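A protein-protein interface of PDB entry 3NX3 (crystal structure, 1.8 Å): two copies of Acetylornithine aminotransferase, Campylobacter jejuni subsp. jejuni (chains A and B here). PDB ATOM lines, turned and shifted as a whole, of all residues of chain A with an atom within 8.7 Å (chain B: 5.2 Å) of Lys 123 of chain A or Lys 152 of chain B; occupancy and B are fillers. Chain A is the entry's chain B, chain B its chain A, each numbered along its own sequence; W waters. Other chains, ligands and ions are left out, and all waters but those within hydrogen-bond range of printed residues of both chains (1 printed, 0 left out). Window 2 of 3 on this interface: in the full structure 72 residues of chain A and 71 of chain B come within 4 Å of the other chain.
Water W1 lies within hydrogen-bond range of the backbone carbonyl oxygen (O) of Lys 155 of chain B, the backbone carbonyl oxygen (O) of Pro 153 of chain B and the backbone NH (N) of Gly 124 of chain A.
The side-chain amino group (NZ) of Lys 123 of chain A sits close to the backbone carbonyl oxygen (O) of Lys 152 of chain B (3.5 Å).
The backbone carbonyl oxygen (O) of Phe 154 of chain B lies within hydrogen-bond range of the guanidinium group (NH1) of Arg 114 of chain A (2.9 Å).
Pro 153 of chain B touches Arg 114 of chain A.
NH1 of Arg 114 of chain A touches C of Lys 155 of chain B, at 3.6 Å.
Lys 115 of chain A touches Phe 154 of chain B (CB to CE1, 3.997 Å).
CZ of Phe 118 of chain A touches CG of Lys 152 of chain B, 3.8 Å away.
Pro 153 of chain B touches Phe 118 of chain A (CB to CD2, 3.5 Å).
Lys 123 of chain A touches Lys 155 of chain B (CE to CB, 3.7 Å).
Gly 124 of chain A touches Lys 155 of chain B (CA to O, 3.3 Å).
No position is printed for both chains.
Of the 9 pairs that touch across the chains among the printed residues, none has its exchanged pair printed and touching as well.
Printed residues of chain A that touch a printed residue of chain B: Arg 114, Lys 115, Phe 118, Lys 123 and Gly 124.
Hydrophobic or aromatic side chains of chain A that line the printed part of chain B: Phe 118.
Printed residues of chain B that touch a printed residue of chain A: Lys 152, Pro 153, Phe 154 and Lys 155.
Hydrophobic or aromatic side chains of chain B within 4 Å of the printed part of chain A: Pro 153 and Phe 154.
Among the printed residues, 9 pairs touch across the chains.
Among the printed residues, no Asp or Glu carboxylate lies within 4 Å of a Lys or Arg side-chain nitrogen of the other chain.
Of the printed residues of chain B, Arg 114 of chain A touches Pro 153, Phe 154 and Lys 155.
Printed residues of chain B within 4 Å of Phe 118 of chain A: Lys 152 (3.8 Å) and Pro 153 (3.5 Å).
Of chain B, only Lys 152 (3.1 Å) and Lys 155 (3.7 Å) come within 4 Å of Lys 123 of chain A.
Lys 152 of chain B touches two residues of chain A.
Of the printed residues of chain A, Pro 153 of chain B touches Arg 114 (3.8 Å) and Phe 118 (3.5 Å).
Of the printed residues of chain A, Phe 154 of chain B touches Arg 114 and Lys 115.
Lys 155 of chain B touches just these residues of chain A: Arg 114, Lys 123 and Gly 124.
The nearest residue of chain B that does not touch Lys 123 of chain A is Pro 153 of chain B (4.9 Å).
The nearest printed residue of chain A that does not touch Phe 154 of chain B is Lys 123 of chain A (5.4 Å).
The backbone carbonyl oxygen (O) of Lys 123 of chain A is in hydrogen-bond range of the side-chain amino group (NZ) of Lys 179 of chain A (2.8 Å).
The backbone carbonyl oxygen (O) of Gly 125 of chain A sits at hydrogen-bond distance from the guanidinium group (NE) of Arg 114 of chain A, 2.7 Å away.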
ATOM      1  N   ARG A 114      18.174  -0.883  14.212  1.00  0.00           N
ATOM      2  CA  ARG A 114      19.218  -0.642  13.223  1.00  0.00           C
ATOM      3  C   ARG A 114      19.819  -1.934  12.713  1.00  0.00           C
ATOM      4  O   ARG A 114      20.083  -2.082  11.529  1.00  0.00           O
ATOM      5  CB  ARG A 114      20.328   0.237  13.779  1.00  0.00           C
ATOM      6  CG  ARG A 114      20.017   1.686  13.687  1.00  0.00           C
ATOM      7  CD  ARG A 114      21.218   2.497  13.295  1.00  0.00           C
ATOM      8  NE  ARG A 114      20.804   3.831  12.897  1.00  0.00           N
ATOM      9  CZ  ARG A 114      21.463   4.937  13.207  1.00  0.00           C
ATOM     10  NH1 ARG A 114      22.568   4.869  13.926  1.00  0.00           N
ATOM     11  NH2 ARG A 114      21.010   6.109  12.807  1.00  0.00           N
ATOM     12  N   LYS A 115      20.051  -2.860  13.631  1.00  0.00           N
ATOM     13  CA  LYS A 115      20.613  -4.148  13.284  1.00  0.00           C
ATOM     14  C   LYS A 115      19.657  -4.931  12.395  1.00  0.00           C
ATOM     15  O   LYS A 115      20.074  -5.611  11.469  1.00  0.00           O
ATOM     16  CB  LYS A 115      20.963  -4.935  14.538  1.00  0.00           C
ATOM     17  CG  LYS A 115      21.794  -6.155  14.269  1.00  0.00           C
ATOM     18  CD  LYS A 115      22.388  -6.694  15.545  1.00  0.00           C
ATOM     19  CE  LYS A 115      23.080  -8.012  15.306  1.00  0.00           C
ATOM     20  NZ  LYS A 115      22.111  -9.039  14.873  1.00  0.00           N
ATOM     21  N   TYR A 116      18.372  -4.840  12.699  1.00  0.00           N
ATOM     22  CA  TYR A 116      17.367  -5.524  11.903  1.00  0.00           C
ATOM     23  C   TYR A 116      17.465  -5.066  10.452  1.00  0.00           C
ATOM     24  O   TYR A 116      17.480  -5.888   9.532  1.00  0.00           O
ATOM     25  CB  TYR A 116      15.973  -5.239  12.459  1.00  0.00           C
ATOM     26  CG  TYR A 116      14.832  -5.815  11.648  1.00  0.00           C
ATOM     27  CD1 TYR A 116      14.338  -7.085  11.919  1.00  0.00           C
ATOM     28  CD2 TYR A 116      14.232  -5.076  10.634  1.00  0.00           C
ATOM     29  CE1 TYR A 116      13.281  -7.612  11.192  1.00  0.00           C
ATOM     30  CE2 TYR A 116      13.182  -5.594   9.898  1.00  0.00           C
ATOM     31  CZ  TYR A 116      12.710  -6.861  10.185  1.00  0.00           C
ATOM     32  OH  TYR A 116      11.662  -7.380   9.461  1.00  0.00           O
ATOM     33  N   ALA A 117      17.530  -3.752  10.250  1.00  0.00           N
ATOM     34  CA  ALA A 117      17.593  -3.190   8.905  1.00  0.00           C
ATOM     35  C   ALA A 117      18.939  -3.519   8.281  1.00  0.00           C
ATOM     36  O   ALA A 117      19.020  -3.864   7.101  1.00  0.00           O
ATOM     37  CB  ALA A 117      17.368  -1.680   8.940  1.00  0.00           C
ATOM     38  N   PHE A 118      19.990  -3.424   9.090  1.00  0.00           N
ATOM     39  CA  PHE A 118      21.344  -3.738   8.647  1.00  0.00           C
ATOM     40  C   PHE A 118      21.437  -5.153   8.048  1.00  0.00           C
ATOM     41  O   PHE A 118      22.048  -5.352   6.998  1.00  0.00           O
ATOM     42  CB  PHE A 118      22.333  -3.570   9.804  1.00  0.00           C
ATOM     43  CG  PHE A 118      23.762  -3.772   9.406  1.00  0.00           C
ATOM     44  CD1 PHE A 118      24.476  -2.749   8.809  1.00  0.00           C
ATOM     45  CD2 PHE A 118      24.389  -4.989   9.617  1.00  0.00           C
ATOM     46  CE1 PHE A 118      25.794  -2.929   8.437  1.00  0.00           C
ATOM     47  CE2 PHE A 118      25.707  -5.179   9.246  1.00  0.00           C
ATOM     48  CZ  PHE A 118      26.411  -4.147   8.654  1.00  0.00           C
ATOM     49  N   ASN A 119      20.822  -6.127   8.716  1.00  0.00           N
ATOM     50  CA  ASN A 119      20.804  -7.501   8.226  1.00  0.00           C
ATOM     51  C   ASN A 119      19.987  -7.676   6.946  1.00  0.00           C
ATOM     52  O   ASN A 119      20.222  -8.607   6.172  1.00  0.00           O
ATOM     53  CB  ASN A 119      20.295  -8.455   9.313  1.00  0.00           C
ATOM     54  CG  ASN A 119      21.264  -8.584  10.473  1.00  0.00           C
ATOM     55  OD1 ASN A 119      22.450  -8.275  10.340  1.00  0.00           O
ATOM     56  ND2 ASN A 119      20.765  -9.046  11.618  1.00  0.00           N
ATOM     57  N   LYS A 120      19.021  -6.788   6.732  1.00  0.00           N
ATOM     58  CA  LYS A 120      18.212  -6.810   5.517  1.00  0.00           C
ATOM     59  C   LYS A 120      18.932  -6.083   4.386  1.00  0.00           C
ATOM     60  O   LYS A 120      18.392  -5.939   3.292  1.00  0.00           O
ATOM     61  CB  LYS A 120      16.850  -6.150   5.755  1.00  0.00           C
ATOM     62  CG  LYS A 120      16.004  -6.791   6.836  1.00  0.00           C
ATOM     63  CD  LYS A 120      15.154  -7.927   6.300  1.00  0.00           C
ATOM     64  CE  LYS A 120      14.200  -8.425   7.368  1.00  0.00           C
ATOM     65  NZ  LYS A 120      13.206  -9.393   6.837  1.00  0.00           N
ATOM     66  N   GLY A 121      20.145  -5.612   4.663  1.00  0.00           N
ATOM     67  CA  GLY A 121      20.938  -4.914   3.670  1.00  0.00           C
ATOM     68  C   GLY A 121      20.847  -3.400   3.725  1.00  0.00           C
ATOM     69  O   GLY A 121      21.452  -2.715   2.901  1.00  0.00           O
ATOM     70  N   VAL A 122      20.102  -2.870   4.693  1.00  0.00           N
ATOM     71  CA  VAL A 122      19.903  -1.426   4.792  1.00  0.00           C
ATOM     72  C   VAL A 122      20.797  -0.813   5.864  1.00  0.00           C
ATOM     73  O   VAL A 122      20.561  -0.988   7.064  1.00  0.00           O
ATOM     74  CB  VAL A 122      18.430  -1.079   5.085  1.00  0.00           C
ATOM     75  CG1 VAL A 122      18.259   0.423   5.233  1.00  0.00           C
ATOM     76  CG2 VAL A 122      17.535  -1.619   3.983  1.00  0.00           C
ATOM     77  N   LYS A 123      21.828  -0.095   5.431  1.00  0.00           N
ATOM     78  CA  LYS A 123      22.796   0.462   6.365  1.00  0.00           C
ATOM     79  C   LYS A 123      22.326   1.815   6.893  1.00  0.00           C
ATOM     80  O   LYS A 123      21.710   2.594   6.166  1.00  0.00           O
ATOM     81  CB  LYS A 123      24.176   0.576   5.706  1.00  0.00           C
ATOM     82  CG  LYS A 123      25.274   1.094   6.627  1.00  0.00           C
ATOM     83  CD  LYS A 123      25.376   0.259   7.898  1.00  0.00           C
ATOM     84  CE  LYS A 123      26.410   0.813   8.876  1.00  0.00           C
ATOM     85  NZ  LYS A 123      27.817   0.592   8.435  1.00  0.00           N
ATOM     86  N   GLY A 124      22.605   2.077   8.165  1.00  0.00           N
ATOM     87  CA  GLY A 124      22.285   3.354   8.778  1.00  0.00           C
ATOM     88  C   GLY A 124      20.799   3.639   8.835  1.00  0.00           C
ATOM     89  O   GLY A 124      20.350   4.709   8.431  1.00  0.00           O
ATOM     90  N   GLY A 125      20.035   2.675   9.336  1.00  0.00           N
ATOM     91  CA  GLY A 125      18.594   2.816   9.450  1.00  0.00           C
ATOM     92  C   GLY A 125      18.197   4.098  10.163  1.00  0.00           C
ATOM     93  O   GLY A 125      18.822   4.485  11.150  1.00  0.00           O
ATOM     94  N   GLN A 126      17.165   4.757   9.649  1.00  0.00           N
ATOM     95  CA  GLN A 126      16.658   5.996  10.235  1.00  0.00           C
ATOM     96  C   GLN A 126      15.435   5.771  11.117  1.00  0.00           C
ATOM     97  O   GLN A 126      14.736   4.765  10.990  1.00  0.00           O
ATOM     98  CB  GLN A 126      16.301   7.000   9.139  1.00  0.00           C
ATOM     99  CG  GLN A 126      17.490   7.542   8.388  1.00  0.00           C
ATOM    100  CD  GLN A 126      17.088   8.507   7.295  1.00  0.00           C
ATOM    101  OE1 GLN A 126      15.900   8.704   7.021  1.00  0.00           O
ATOM    102  NE2 GLN A 126      18.079   9.119   6.661  1.00  0.00           N
ATOM    103  N   ASN A 177      11.115   6.840   4.131  1.00  0.00           N
ATOM    104  CA  ASN A 177      11.897   6.608   2.925  1.00  0.00           C
ATOM    105  C   ASN A 177      12.575   5.249   2.998  1.00  0.00           C
ATOM    106  O   ASN A 177      12.344   4.487   3.938  1.00  0.00           O
ATOM    107  CB  ASN A 177      12.932   7.711   2.725  1.00  0.00           C
ATOM    108  CG  ASN A 177      13.849   7.861   3.912  1.00  0.00           C
ATOM    109  OD1 ASN A 177      14.622   6.956   4.229  1.00  0.00           O
ATOM    110  ND2 ASN A 177      13.768   9.006   4.585  1.00  0.00           N
ATOM    111  N   GLU A 178      13.414   4.953   2.008  1.00  0.00           N
ATOM    112  CA  GLU A 178      14.092   3.659   1.925  1.00  0.00           C
ATOM    113  C   GLU A 178      15.010   3.363   3.117  1.00  0.00           C
ATOM    114  O   GLU A 178      15.375   2.211   3.350  1.00  0.00           O
ATOM    115  CB  GLU A 178      14.886   3.555   0.620  1.00  0.00           C
ATOM    116  CG  GLU A 178      14.022   3.425  -0.625  1.00  0.00           C
ATOM    117  CD  GLU A 178      13.295   2.093  -0.699  1.00  0.00           C
ATOM    118  OE1 GLU A 178      13.673   1.161   0.046  1.00  0.00           O
ATOM    119  OE2 GLU A 178      12.345   1.978  -1.502  1.00  0.00           O
ATOM    120  N   LYS A 179      15.376   4.393   3.872  1.00  0.00           N
ATOM    121  CA  LYS A 179      16.283   4.201   5.004  1.00  0.00           C
ATOM    122  C   LYS A 179      15.569   4.074   6.353  1.00  0.00           C
ATOM    123  O   LYS A 179      16.195   3.712   7.342  1.00  0.00           O
ATOM    124  CB  LYS A 179      17.326   5.320   5.071  1.00  0.00           C
ATOM    125  CG  LYS A 179      18.065   5.568   3.764  1.00  0.00           C
ATOM    126  CD  LYS A 179      18.834   4.341   3.289  1.00  0.00           C
ATOM    127  CE  LYS A 179      20.060   4.082   4.150  1.00  0.00           C
ATOM    128  NZ  LYS A 179      20.974   3.072   3.537  1.00  0.00           N
ATOM    129  N   THR A 180      14.270   4.372   6.393  1.00  0.00           N
ATOM    130  CA  THR A 180      13.514   4.289   7.643  1.00  0.00           C
ATOM    131  C   THR A 180      13.511   2.852   8.150  1.00  0.00           C
ATOM    132  O   THR A 180      13.098   1.940   7.436  1.00  0.00           O
ATOM    133  CB  THR A 180      12.045   4.746   7.479  1.00  0.00           C
ATOM    134  OG1 THR A 180      11.988   5.975   6.744  1.00  0.00           O
ATOM    135  CG2 THR A 180      11.403   4.953   8.841  1.00  0.00           C
ATOM    136  N   CYS A 181      13.973   2.649   9.382  1.00  0.00           N
ATOM    137  CA  CYS A 181      14.002   1.307   9.946  1.00  0.00           C
ATOM    138  C   CYS A 181      13.005   1.162  11.093  1.00  0.00           C
ATOM    139  O   CYS A 181      12.583   0.057  11.412  1.00  0.00           O
ATOM    140  CB  CYS A 181      15.422   0.924  10.389  1.00  0.00           C
ATOM    141  SG  CYS A 181      15.986   1.649  11.945  1.00  0.00           S
ATOM    142  N   GLU B 148      35.672  -1.699  15.227  1.00  0.00           N
ATOM    143  CA  GLU B 148      34.592  -1.577  14.257  1.00  0.00           C
ATOM    144  C   GLU B 148      33.569  -2.697  14.406  1.00  0.00           C
ATOM    145  O   GLU B 148      32.415  -2.543  14.013  1.00  0.00           O
ATOM    146  CB  GLU B 148      35.146  -1.538  12.831  1.00  0.00           C
ATOM    147  CG  GLU B 148      35.734  -0.190  12.439  1.00  0.00           C
ATOM    148  CD  GLU B 148      36.551  -0.254  11.165  1.00  0.00           C
ATOM    149  OE1 GLU B 148      36.069   0.231  10.118  1.00  0.00           O
ATOM    150  OE2 GLU B 148      37.681  -0.784  11.212  1.00  0.00           O
ATOM    151  N   LYS B 149      33.995  -3.814  14.986  1.00  0.00           N
ATOM    152  CA  LYS B 149      33.117  -4.966  15.170  1.00  0.00           C
ATOM    153  C   LYS B 149      31.942  -4.682  16.102  1.00  0.00           C
ATOM    154  O   LYS B 149      30.829  -5.145  15.859  1.00  0.00           O
ATOM    155  CB  LYS B 149      33.903  -6.174  15.688  1.00  0.00           C
ATOM    156  CG  LYS B 149      33.032  -7.396  15.948  1.00  0.00           C
ATOM    157  CD  LYS B 149      33.836  -8.575  16.478  1.00  0.00           C
ATOM    158  CE  LYS B 149      34.382  -8.299  17.870  1.00  0.00           C
ATOM    159  NZ  LYS B 149      35.105  -9.483  18.416  1.00  0.00           N
ATOM    160  N   TYR B 150      32.195  -3.934  17.173  1.00  0.00           N
ATOM    161  CA  TYR B 150      31.164  -3.635  18.163  1.00  0.00           C
ATOM    162  C   TYR B 150      30.194  -2.579  17.655  1.00  0.00           C
ATOM    163  O   TYR B 150      29.130  -2.368  18.234  1.00  0.00           O
ATOM    164  CB  TYR B 150      31.793  -3.130  19.465  1.00  0.00           C
ATOM    165  CG  TYR B 150      32.649  -4.143  20.185  1.00  0.00           C
ATOM    166  CD1 TYR B 150      32.104  -4.983  21.147  1.00  0.00           C
ATOM    167  CD2 TYR B 150      34.004  -4.254  19.910  1.00  0.00           C
ATOM    168  CE1 TYR B 150      32.886  -5.910  21.809  1.00  0.00           C
ATOM    169  CE2 TYR B 150      34.793  -5.176  20.566  1.00  0.00           C
ATOM    170  CZ  TYR B 150      34.229  -6.001  21.514  1.00  0.00           C
ATOM    171  OH  TYR B 150      35.012  -6.924  22.166  1.00  0.00           O
ATOM    172  N   GLN B 151      30.573  -1.910  16.576  1.00  0.00           N
ATOM    173  CA  GLN B 151      29.831  -0.744  16.111  1.00  0.00           C
ATOM    174  C   GLN B 151      29.064  -0.999  14.824  1.00  0.00           C
ATOM    175  O   GLN B 151      27.984  -0.446  14.617  1.00  0.00           O
ATOM    176  CB  GLN B 151      30.795   0.417  15.884  1.00  0.00           C
ATOM    177  CG  GLN B 151      31.542   0.854  17.133  1.00  0.00           C
ATOM    178  CD  GLN B 151      32.454   2.032  16.859  1.00  0.00           C
ATOM    179  OE1 GLN B 151      33.032   2.141  15.778  1.00  0.00           O
ATOM    180  NE2 GLN B 151      32.577   2.932  17.832  1.00  0.00           N
ATOM    181  N   LYS B 152      29.637  -1.839  13.969  1.00  0.00           N
ATOM    182  CA  LYS B 152      29.241  -1.934  12.565  1.00  0.00           C
ATOM    183  C   LYS B 152      27.741  -1.808  12.269  1.00  0.00           C
ATOM    184  O   LYS B 152      27.329  -0.881  11.571  1.00  0.00           O
ATOM    185  CB  LYS B 152      29.826  -3.198  11.916  1.00  0.00           C
ATOM    186  CG  LYS B 152      29.645  -3.256  10.407  1.00  0.00           C
ATOM    187  CD  LYS B 152      30.226  -2.016   9.739  1.00  0.00           C
ATOM    188  CE  LYS B 152      29.999  -2.036   8.230  1.00  0.00           C
ATOM    189  NZ  LYS B 152      30.496  -0.795   7.568  1.00  0.00           N
ATOM    190  N   PRO B 153      26.920  -2.741  12.780  1.00  0.00           N
ATOM    191  CA  PRO B 153      25.503  -2.682  12.402  1.00  0.00           C
ATOM    192  C   PRO B 153      24.743  -1.469  12.956  1.00  0.00           C
ATOM    193  O   PRO B 153      23.660  -1.170  12.458  1.00  0.00           O
ATOM    194  CB  PRO B 153      24.929  -3.991  12.963  1.00  0.00           C
ATOM    195  CG  PRO B 153      25.880  -4.398  14.037  1.00  0.00           C
ATOM    196  CD  PRO B 153      27.231  -3.931  13.592  1.00  0.00           C
ATOM    197  N   PHE B 154      25.308  -0.770  13.938  1.00  0.00           N
ATOM    198  CA  PHE B 154      24.592   0.313  14.610  1.00  0.00           C
ATOM    199  C   PHE B 154      24.955   1.711  14.108  1.00  0.00           C
ATOM    200  O   PHE B 154      24.366   2.696  14.550  1.00  0.00           O
ATOM    201  CB  PHE B 154      24.837   0.244  16.117  1.00  0.00           C
ATOM    202  CG  PHE B 154      24.682  -1.128  16.680  1.00  0.00           C
ATOM    203  CD1 PHE B 154      23.446  -1.760  16.656  1.00  0.00           C
ATOM    204  CD2 PHE B 154      25.766  -1.794  17.217  1.00  0.00           C
ATOM    205  CE1 PHE B 154      23.290  -3.035  17.175  1.00  0.00           C
ATOM    206  CE2 PHE B 154      25.620  -3.076  17.734  1.00  0.00           C
ATOM    207  CZ  PHE B 154      24.375  -3.694  17.713  1.00  0.00           C
ATOM    208  N   LYS B 155      25.927   1.792  13.204  1.00  0.00           N
ATOM    209  CA  LYS B 155      26.366   3.073  12.654  1.00  0.00           C
ATOM    210  C   LYS B 155      25.256   3.732  11.835  1.00  0.00           C
ATOM    211  O   LYS B 155      24.391   3.050  11.292  1.00  0.00           O
ATOM    212  CB  LYS B 155      27.597   2.874  11.767  1.00  0.00           C
ATOM    213  CG  LYS B 155      28.866   2.490  12.508  1.00  0.00           C
ATOM    214  CD  LYS B 155      29.990   2.214  11.521  1.00  0.00           C
ATOM    215  CE  LYS B 155      31.278   1.827  12.230  1.00  0.00           C
ATOM    216  NZ  LYS B 155      32.340   1.408  11.266  1.00  0.00           N
HETATM  217  O   HOH W   1      23.937   0.654  10.435  1.00  0.00           O
